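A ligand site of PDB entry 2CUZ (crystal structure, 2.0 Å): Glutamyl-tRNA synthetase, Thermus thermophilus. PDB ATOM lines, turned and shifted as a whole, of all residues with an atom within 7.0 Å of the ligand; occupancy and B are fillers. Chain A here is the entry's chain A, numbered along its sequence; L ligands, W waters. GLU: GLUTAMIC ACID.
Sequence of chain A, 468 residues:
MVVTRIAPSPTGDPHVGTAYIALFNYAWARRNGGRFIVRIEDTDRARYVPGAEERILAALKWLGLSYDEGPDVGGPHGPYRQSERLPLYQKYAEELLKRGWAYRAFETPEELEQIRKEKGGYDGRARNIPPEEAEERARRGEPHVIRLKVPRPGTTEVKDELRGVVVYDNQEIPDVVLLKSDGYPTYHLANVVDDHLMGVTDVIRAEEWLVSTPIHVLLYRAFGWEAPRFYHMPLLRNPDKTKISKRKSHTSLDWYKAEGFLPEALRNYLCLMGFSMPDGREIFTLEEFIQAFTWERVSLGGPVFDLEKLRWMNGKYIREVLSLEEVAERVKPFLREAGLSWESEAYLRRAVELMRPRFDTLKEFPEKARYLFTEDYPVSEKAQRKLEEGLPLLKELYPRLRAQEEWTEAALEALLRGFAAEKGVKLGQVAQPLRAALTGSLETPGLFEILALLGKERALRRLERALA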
ATOM      1  N   ARG A   5     -13.980  24.080 -10.254  1.00  0.00           N
ATOM      2  CA  ARG A   5     -15.324  23.683 -10.568  1.00  0.00           C
ATOM      3  C   ARG A   5     -16.122  23.275  -9.349  1.00  0.00           C
ATOM      4  O   ARG A   5     -15.541  23.050  -8.283  1.00  0.00           O
ATOM      5  CB  ARG A   5     -15.343  22.534 -11.584  1.00  0.00           C
ATOM      6  CG  ARG A   5     -14.345  21.400 -11.342  1.00  0.00           C
ATOM      7  CD  ARG A   5     -14.298  20.907  -9.933  1.00  0.00           C
ATOM      8  NE  ARG A   5     -13.763  19.542  -9.863  1.00  0.00           N
ATOM      9  CZ  ARG A   5     -14.027  18.720  -8.869  1.00  0.00           C
ATOM     10  NH1 ARG A   5     -14.791  19.140  -7.853  1.00  0.00           N
ATOM     11  NH2 ARG A   5     -13.594  17.460  -8.915  1.00  0.00           N
ATOM     12  N   ILE A   6     -17.438  23.255  -9.502  1.00  0.00           N
ATOM     13  CA  ILE A   6     -18.321  22.732  -8.481  1.00  0.00           C
ATOM     14  C   ILE A   6     -18.915  21.551  -9.267  1.00  0.00           C
ATOM     15  O   ILE A   6     -19.148  21.673 -10.473  1.00  0.00           O
ATOM     16  CB  ILE A   6     -19.399  23.738  -8.033  1.00  0.00           C
ATOM     17  CG1 ILE A   6     -20.192  23.102  -6.889  1.00  0.00           C
ATOM     18  CG2 ILE A   6     -20.329  24.132  -9.199  1.00  0.00           C
ATOM     19  CD1 ILE A   6     -21.498  23.839  -6.634  1.00  0.00           C
ATOM     20  N   ALA A   7     -19.114  20.399  -8.627  1.00  0.00           N
ATOM     21  CA  ALA A   7     -19.608  19.219  -9.360  1.00  0.00           C
ATOM     22  C   ALA A   7     -20.728  18.522  -8.612  1.00  0.00           C
ATOM     23  O   ALA A   7     -20.570  17.386  -8.136  1.00  0.00           O
ATOM     24  CB  ALA A   7     -18.430  18.243  -9.604  1.00  0.00           C
ATOM     25  N   PRO A   8     -21.904  19.174  -8.540  1.00  0.00           N
ATOM     26  CA  PRO A   8     -23.078  18.664  -7.849  1.00  0.00           C
ATOM     27  C   PRO A   8     -23.783  17.495  -8.498  1.00  0.00           C
ATOM     28  O   PRO A   8     -23.792  17.366  -9.726  1.00  0.00           O
ATOM     29  CB  PRO A   8     -23.985  19.888  -7.735  1.00  0.00           C
ATOM     30  CG  PRO A   8     -23.685  20.648  -8.993  1.00  0.00           C
ATOM     31  CD  PRO A   8     -22.207  20.393  -9.306  1.00  0.00           C
ATOM     32  N   SER A   9     -24.343  16.635  -7.640  1.00  0.00           N
ATOM     33  CA  SER A   9     -25.101  15.468  -8.066  1.00  0.00           C
ATOM     34  C   SER A   9     -26.553  15.871  -7.855  1.00  0.00           C
ATOM     35  O   SER A   9     -26.925  16.270  -6.764  1.00  0.00           O
ATOM     36  CB  SER A   9     -24.764  14.256  -7.213  1.00  0.00           C
ATOM     37  OG  SER A   9     -23.426  13.827  -7.465  1.00  0.00           O
ATOM     38  N   PRO A  10     -27.365  15.827  -8.909  1.00  0.00           N
ATOM     39  CA  PRO A  10     -28.762  16.213  -8.773  1.00  0.00           C
ATOM     40  C   PRO A  10     -29.620  15.064  -8.215  1.00  0.00           C
ATOM     41  O   PRO A  10     -30.443  14.469  -8.923  1.00  0.00           O
ATOM     42  CB  PRO A  10     -29.139  16.577 -10.202  1.00  0.00           C
ATOM     43  CG  PRO A  10     -28.395  15.539 -10.987  1.00  0.00           C
ATOM     44  CD  PRO A  10     -27.031  15.521 -10.313  1.00  0.00           C
ATOM     45  N   THR A  11     -29.450  14.778  -6.929  1.00  0.00           N
ATOM     46  CA  THR A  11     -30.174  13.693  -6.280  1.00  0.00           C
ATOM     47  C   THR A  11     -31.068  14.139  -5.124  1.00  0.00           C
ATOM     48  O   THR A  11     -31.604  13.301  -4.387  1.00  0.00           O
ATOM     49  CB  THR A  11     -29.191  12.698  -5.741  1.00  0.00           C
ATOM     50  OG1 THR A  11     -28.391  13.355  -4.764  1.00  0.00           O
ATOM     51  CG2 THR A  11     -28.293  12.178  -6.871  1.00  0.00           C
ATOM     52  N   THR A  18     -23.184  22.290  -0.745  1.00  0.00           N
ATOM     53  CA  THR A  18     -22.727  22.496  -2.114  1.00  0.00           C
ATOM     54  C   THR A  18     -22.416  23.986  -2.294  1.00  0.00           C
ATOM     55  O   THR A  18     -21.458  24.358  -2.981  1.00  0.00           O
ATOM     56  CB  THR A  18     -23.783  22.044  -3.115  1.00  0.00           C
ATOM     57  OG1 THR A  18     -24.066  20.663  -2.870  1.00  0.00           O
ATOM     58  CG2 THR A  18     -23.278  22.217  -4.543  1.00  0.00           C
ATOM     59  N   ILE A  21     -19.001  24.736  -0.659  1.00  0.00           N
ATOM     60  CA  ILE A  21     -17.907  24.341  -1.544  1.00  0.00           C
ATOM     61  C   ILE A  21     -17.860  25.265  -2.784  1.00  0.00           C
ATOM     62  O   ILE A  21     -16.778  25.698  -3.204  1.00  0.00           O
ATOM     63  CB  ILE A  21     -18.060  22.887  -2.003  1.00  0.00           C
ATOM     64  CG1 ILE A  21     -18.003  21.958  -0.778  1.00  0.00           C
ATOM     65  CG2 ILE A  21     -16.951  22.511  -2.992  1.00  0.00           C
ATOM     66  CD1 ILE A  21     -16.729  22.071   0.016  1.00  0.00           C
ATOM     67  N   ARG A  39     -20.102  21.325 -13.349  1.00  0.00           N
ATOM     68  CA  ARG A  39     -20.265  20.034 -14.007  1.00  0.00           C
ATOM     69  C   ARG A  39     -21.297  19.209 -13.208  1.00  0.00           C
ATOM     70  O   ARG A  39     -21.107  18.950 -12.021  1.00  0.00           O
ATOM     71  CB  ARG A  39     -18.906  19.280 -14.135  1.00  0.00           C
ATOM     72  CG  ARG A  39     -19.094  17.847 -14.678  1.00  0.00           C
ATOM     73  CD  ARG A  39     -17.752  17.103 -14.848  1.00  0.00           C
ATOM     74  NE  ARG A  39     -17.150  16.765 -13.560  1.00  0.00           N
ATOM     75  CZ  ARG A  39     -15.958  17.182 -13.141  1.00  0.00           C
ATOM     76  NH1 ARG A  39     -15.219  17.988 -13.913  1.00  0.00           N
ATOM     77  NH2 ARG A  39     -15.486  16.779 -11.953  1.00  0.00           N
ATOM     78  N   ILE A  40     -22.377  18.798 -13.874  1.00  0.00           N
ATOM     79  CA  ILE A  40     -23.432  18.029 -13.216  1.00  0.00           C
ATOM     80  C   ILE A  40     -23.056  16.548 -13.234  1.00  0.00           C
ATOM     81  O   ILE A  40     -22.818  15.985 -14.293  1.00  0.00           O
ATOM     82  CB  ILE A  40     -24.810  18.207 -13.930  1.00  0.00           C
ATOM     83  CG1 ILE A  40     -25.233  19.681 -13.882  1.00  0.00           C
ATOM     84  CG2 ILE A  40     -25.904  17.319 -13.253  1.00  0.00           C
ATOM     85  CD1 ILE A  40     -25.525  20.175 -12.474  1.00  0.00           C
ATOM     86  N   GLU A  41     -22.982  15.938 -12.055  1.00  0.00           N
ATOM     87  CA  GLU A  41     -22.605  14.525 -11.972  1.00  0.00           C
ATOM     88  C   GLU A  41     -23.917  13.781 -11.739  1.00  0.00           C
ATOM     89  O   GLU A  41     -24.342  13.537 -10.597  1.00  0.00           O
ATOM     90  CB  GLU A  41     -21.603  14.319 -10.843  1.00  0.00           C
ATOM     91  CG  GLU A  41     -20.435  15.265 -11.008  1.00  0.00           C
ATOM     92  CD  GLU A  41     -19.133  14.743 -10.394  1.00  0.00           C
ATOM     93  OE1 GLU A  41     -19.171  14.016  -9.394  1.00  0.00           O
ATOM     94  OE2 GLU A  41     -18.069  15.092 -10.915  1.00  0.00           O
ATOM     95  N   GLN A  82     -22.481  14.619 -16.803  1.00  0.00           N
ATOM     96  CA  GLN A  82     -21.770  13.355 -17.013  1.00  0.00           C
ATOM     97  C   GLN A  82     -22.664  12.313 -17.719  1.00  0.00           C
ATOM     98  O   GLN A  82     -22.156  11.422 -18.379  1.00  0.00           O
ATOM     99  CB  GLN A  82     -21.216  12.843 -15.673  1.00  0.00           C
ATOM    100  CG  GLN A  82     -20.175  13.825 -15.047  1.00  0.00           C
ATOM    101  CD  GLN A  82     -19.351  13.201 -13.866  1.00  0.00           C
ATOM    102  OE1 GLN A  82     -18.134  13.311 -13.831  1.00  0.00           O
ATOM    103  NE2 GLN A  82     -20.031  12.553 -12.938  1.00  0.00           N
ATOM    104  N   TYR A 187     -17.415   7.260  -9.521  1.00  0.00           N
ATOM    105  CA  TYR A 187     -16.908   8.606  -9.278  1.00  0.00           C
ATOM    106  C   TYR A 187     -15.400   8.708  -9.570  1.00  0.00           C
ATOM    107  O   TYR A 187     -14.945   9.675 -10.172  1.00  0.00           O
ATOM    108  CB  TYR A 187     -17.129   8.954  -7.787  1.00  0.00           C
ATOM    109  CG  TYR A 187     -16.394  10.184  -7.363  1.00  0.00           C
ATOM    110  CD1 TYR A 187     -16.849  11.458  -7.735  1.00  0.00           C
ATOM    111  CD2 TYR A 187     -15.222  10.097  -6.641  1.00  0.00           C
ATOM    112  CE1 TYR A 187     -16.136  12.623  -7.389  1.00  0.00           C
ATOM    113  CE2 TYR A 187     -14.502  11.242  -6.294  1.00  0.00           C
ATOM    114  CZ  TYR A 187     -14.955  12.502  -6.667  1.00  0.00           C
ATOM    115  OH  TYR A 187     -14.232  13.618  -6.323  1.00  0.00           O
ATOM    116  N   ASN A 191     -14.310  11.574 -12.193  1.00  0.00           N
ATOM    117  CA  ASN A 191     -13.763  12.848 -11.702  1.00  0.00           C
ATOM    118  C   ASN A 191     -12.451  13.138 -12.375  1.00  0.00           C
ATOM    119  O   ASN A 191     -12.200  14.272 -12.808  1.00  0.00           O
ATOM    120  CB  ASN A 191     -13.664  12.893 -10.155  1.00  0.00           C
ATOM    121  CG  ASN A 191     -12.285  12.468  -9.600  1.00  0.00           C
ATOM    122  OD1 ASN A 191     -11.408  13.301  -9.297  1.00  0.00           O
ATOM    123  ND2 ASN A 191     -12.101  11.168  -9.442  1.00  0.00           N
ATOM    124  N   ASP A 195     -12.051  16.252 -14.924  1.00  0.00           N
ATOM    125  CA  ASP A 195     -11.272  17.387 -14.445  1.00  0.00           C
ATOM    126  C   ASP A 195     -10.135  17.605 -15.436  1.00  0.00           C
ATOM    127  O   ASP A 195      -9.723  18.755 -15.704  1.00  0.00           O
ATOM    128  CB  ASP A 195     -10.690  17.133 -13.031  1.00  0.00           C
ATOM    129  CG  ASP A 195     -11.704  17.412 -11.928  1.00  0.00           C
ATOM    130  OD1 ASP A 195     -11.472  17.000 -10.753  1.00  0.00           O
ATOM    131  OD2 ASP A 195     -12.754  18.031 -12.203  1.00  0.00           O
ATOM    132  N   VAL A 203      -8.607  21.578  -7.670  1.00  0.00           N
ATOM    133  CA  VAL A 203      -9.734  20.793  -7.256  1.00  0.00           C
ATOM    134  C   VAL A 203      -9.968  21.121  -5.785  1.00  0.00           C
ATOM    135  O   VAL A 203      -9.172  20.728  -4.927  1.00  0.00           O
ATOM    136  CB  VAL A 203      -9.430  19.264  -7.409  1.00  0.00           C
ATOM    137  CG1 VAL A 203     -10.578  18.414  -6.799  1.00  0.00           C
ATOM    138  CG2 VAL A 203      -9.270  18.923  -8.875  1.00  0.00           C
ATOM    139  N   ILE A 204     -11.050  21.852  -5.516  1.00  0.00           N
ATOM    140  CA  ILE A 204     -11.432  22.243  -4.146  1.00  0.00           C
ATOM    141  C   ILE A 204     -12.738  21.489  -3.878  1.00  0.00           C
ATOM    142  O   ILE A 204     -13.764  21.784  -4.506  1.00  0.00           O
ATOM    143  CB  ILE A 204     -11.678  23.782  -4.042  1.00  0.00           C
ATOM    144  CG1 ILE A 204     -10.433  24.571  -4.485  1.00  0.00           C
ATOM    145  CG2 ILE A 204     -12.111  24.171  -2.620  1.00  0.00           C
ATOM    146  CD1 ILE A 204     -10.753  26.054  -4.847  1.00  0.00           C
ATOM    147  N   ARG A 205     -12.711  20.524  -2.946  1.00  0.00           N
ATOM    148  CA  ARG A 205     -13.886  19.706  -2.652  1.00  0.00           C
ATOM    149  C   ARG A 205     -13.986  19.363  -1.151  1.00  0.00           C
ATOM    150  O   ARG A 205     -13.112  19.723  -0.349  1.00  0.00           O
ATOM    151  CB  ARG A 205     -13.860  18.428  -3.505  1.00  0.00           C
ATOM    152  CG  ARG A 205     -12.591  17.582  -3.364  1.00  0.00           C
ATOM    153  CD  ARG A 205     -12.578  16.388  -4.347  1.00  0.00           C
ATOM    154  NE  ARG A 205     -11.420  15.537  -4.162  1.00  0.00           N
ATOM    155  CZ  ARG A 205     -10.947  14.683  -5.062  1.00  0.00           C
ATOM    156  NH1 ARG A 205     -11.562  14.559  -6.230  1.00  0.00           N
ATOM    157  NH2 ARG A 205      -9.861  13.961  -4.805  1.00  0.00           N
ATOM    158  N   ALA A 206     -15.045  18.653  -0.793  1.00  0.00           N
ATOM    159  CA  ALA A 206     -15.317  18.322   0.609  1.00  0.00           C
ATOM    160  C   ALA A 206     -14.309  17.347   1.254  1.00  0.00           C
ATOM    161  O   ALA A 206     -13.721  16.500   0.575  1.00  0.00           O
ATOM    162  CB  ALA A 206     -16.756  17.768   0.712  1.00  0.00           C
ATOM    163  N   GLU A 208     -14.599  14.717   3.009  1.00  0.00           N
ATOM    164  CA  GLU A 208     -14.902  13.314   2.775  1.00  0.00           C
ATOM    165  C   GLU A 208     -14.141  12.720   1.574  1.00  0.00           C
ATOM    166  O   GLU A 208     -13.936  11.522   1.519  1.00  0.00           O
ATOM    167  CB  GLU A 208     -16.394  13.117   2.492  1.00  0.00           C
ATOM    168  CG  GLU A 208     -17.324  13.747   3.497  1.00  0.00           C
ATOM    169  CD  GLU A 208     -17.540  15.238   3.270  1.00  0.00           C
ATOM    170  OE1 GLU A 208     -16.640  16.042   3.592  1.00  0.00           O
ATOM    171  OE2 GLU A 208     -18.616  15.616   2.764  1.00  0.00           O
ATOM    172  N   TRP A 209     -13.714  13.544   0.619  1.00  0.00           N
ATOM    173  CA  TRP A 209     -13.014  13.014  -0.559  1.00  0.00           C
ATOM    174  C   TRP A 209     -11.532  12.864  -0.366  1.00  0.00           C
ATOM    175  O   TRP A 209     -10.866  12.221  -1.169  1.00  0.00           O
ATOM    176  CB  TRP A 209     -13.278  13.914  -1.783  1.00  0.00           C
ATOM    177  CG  TRP A 209     -14.726  13.989  -2.117  1.00  0.00           C
ATOM    178  CD1 TRP A 209     -15.568  15.043  -1.892  1.00  0.00           C
ATOM    179  CD2 TRP A 209     -15.538  12.929  -2.658  1.00  0.00           C
ATOM    180  NE1 TRP A 209     -16.858  14.698  -2.250  1.00  0.00           N
ATOM    181  CE2 TRP A 209     -16.857  13.406  -2.719  1.00  0.00           C
ATOM    182  CE3 TRP A 209     -15.266  11.618  -3.080  1.00  0.00           C
ATOM    183  CZ2 TRP A 209     -17.921  12.628  -3.203  1.00  0.00           C
ATOM    184  CZ3 TRP A 209     -16.334  10.838  -3.555  1.00  0.00           C
ATOM    185  CH2 TRP A 209     -17.632  11.352  -3.612  1.00  0.00           C
ATOM    186  N   HIS A 216      -7.188   8.706  -7.171  1.00  0.00           N
ATOM    187  CA  HIS A 216      -7.135   9.685  -8.241  1.00  0.00           C
ATOM    188  C   HIS A 216      -5.723   9.945  -8.753  1.00  0.00           C
ATOM    189  O   HIS A 216      -5.512  10.015  -9.951  1.00  0.00           O
ATOM    190  CB  HIS A 216      -7.850  10.966  -7.781  1.00  0.00           C
ATOM    191  CG  HIS A 216      -9.235  10.696  -7.290  1.00  0.00           C
ATOM    192  ND1 HIS A 216      -9.944  11.571  -6.488  1.00  0.00           N
ATOM    193  CD2 HIS A 216     -10.032   9.613  -7.463  1.00  0.00           C
ATOM    194  CE1 HIS A 216     -11.113  11.023  -6.186  1.00  0.00           C
ATOM    195  NE2 HIS A 216     -11.189   9.845  -6.771  1.00  0.00           N
HETATM  196  N   GLU L   1     -20.626  15.005  -7.156  1.00  0.00           N
HETATM  197  CA  GLU L   1     -20.001  14.960  -5.803  1.00  0.00           C
HETATM  198  C   GLU L   1     -20.961  15.224  -4.651  1.00  0.00           C
HETATM  199  O   GLU L   1     -20.583  14.884  -3.514  1.00  0.00           O
HETATM  200  CB  GLU L   1     -18.811  15.941  -5.735  1.00  0.00           C
HETATM  201  CG  GLU L   1     -17.542  15.458  -6.463  1.00  0.00           C
HETATM  202  CD  GLU L   1     -16.314  16.355  -6.251  1.00  0.00           C
HETATM  203  OE1 GLU L   1     -15.200  15.983  -6.657  1.00  0.00           O
HETATM  204  OE2 GLU L   1     -16.472  17.459  -5.674  1.00  0.00           O
HETATM  205  OXT GLU L   1     -22.072  15.761  -4.867  1.00  0.00           O
HETATM  206  O   HOH W   1     -17.951  19.872  -6.086  1.00  0.00           O
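N of the ligand is in hydrogen-bond range of O of Ala 7.
OH of Tyr 187 is in hydrogen-bond range of OE1 of the ligand.
OE1 of Glu 41 lies within salt-bridge range of N of the ligand (2.8 Å).
The side-chain hydroxyl (OG) of Ser 9 lies within hydrogen-bond range of a nitrogen (N) of the ligand.
NH2 of Arg 5 is in salt-bridge range of OE1 of the ligand (3.1 Å).
NH1 of Arg 205 lies within salt-bridge range of OE1 of the ligand (3.9 Å).
The side-chain hydroxyl (OH) of Tyr 187 is in hydrogen-bond range of the guanidinium group (NH1) of Arg 205 (2.8 Å).
O of Tyr 187 lies within hydrogen-bond range of ND2 of Asn 191.
The side-chain hydroxyl of Ser 9 lies close to the backbone carbonyl oxygen of Glu 41 (3.3 Å).
O of Pro 8 lies within hydrogen-bond range of N of Glu 41, 2.8 Å away.
NH2 of Arg 39 lies within salt-bridge range of OE2 of Glu 41, 3.3 Å away.
OE1 of Gln 82 lies close to OE2 of Glu 41.
The guanidinium group (NH2) of Arg 5 lies within salt-bridge range of the side-chain carboxylate (OD1) of Asp 195.
The guanidinium group (NH1) of Arg 205 is in hydrogen-bond range of the side-chain amide oxygen (OD1) of Asn 191.
Trp 209 touches the ligand.
Hydrophobic or aromatic side chains that line the ligand: Tyr 187 and Trp 209.
Of the 23 residues printed, 7 come within 4 Å of the ligand.
Along chain A the residues within 4 Å of the ligand span positions 5 to 209.
The nearest printed residue that does not touch the ligand is Pro 8 (4.2 Å).
Water W1 bridges the backbone NH (N) of Ala 7 (2.8 Å) and an oxygen (OE2) of the ligand (2.9 Å).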
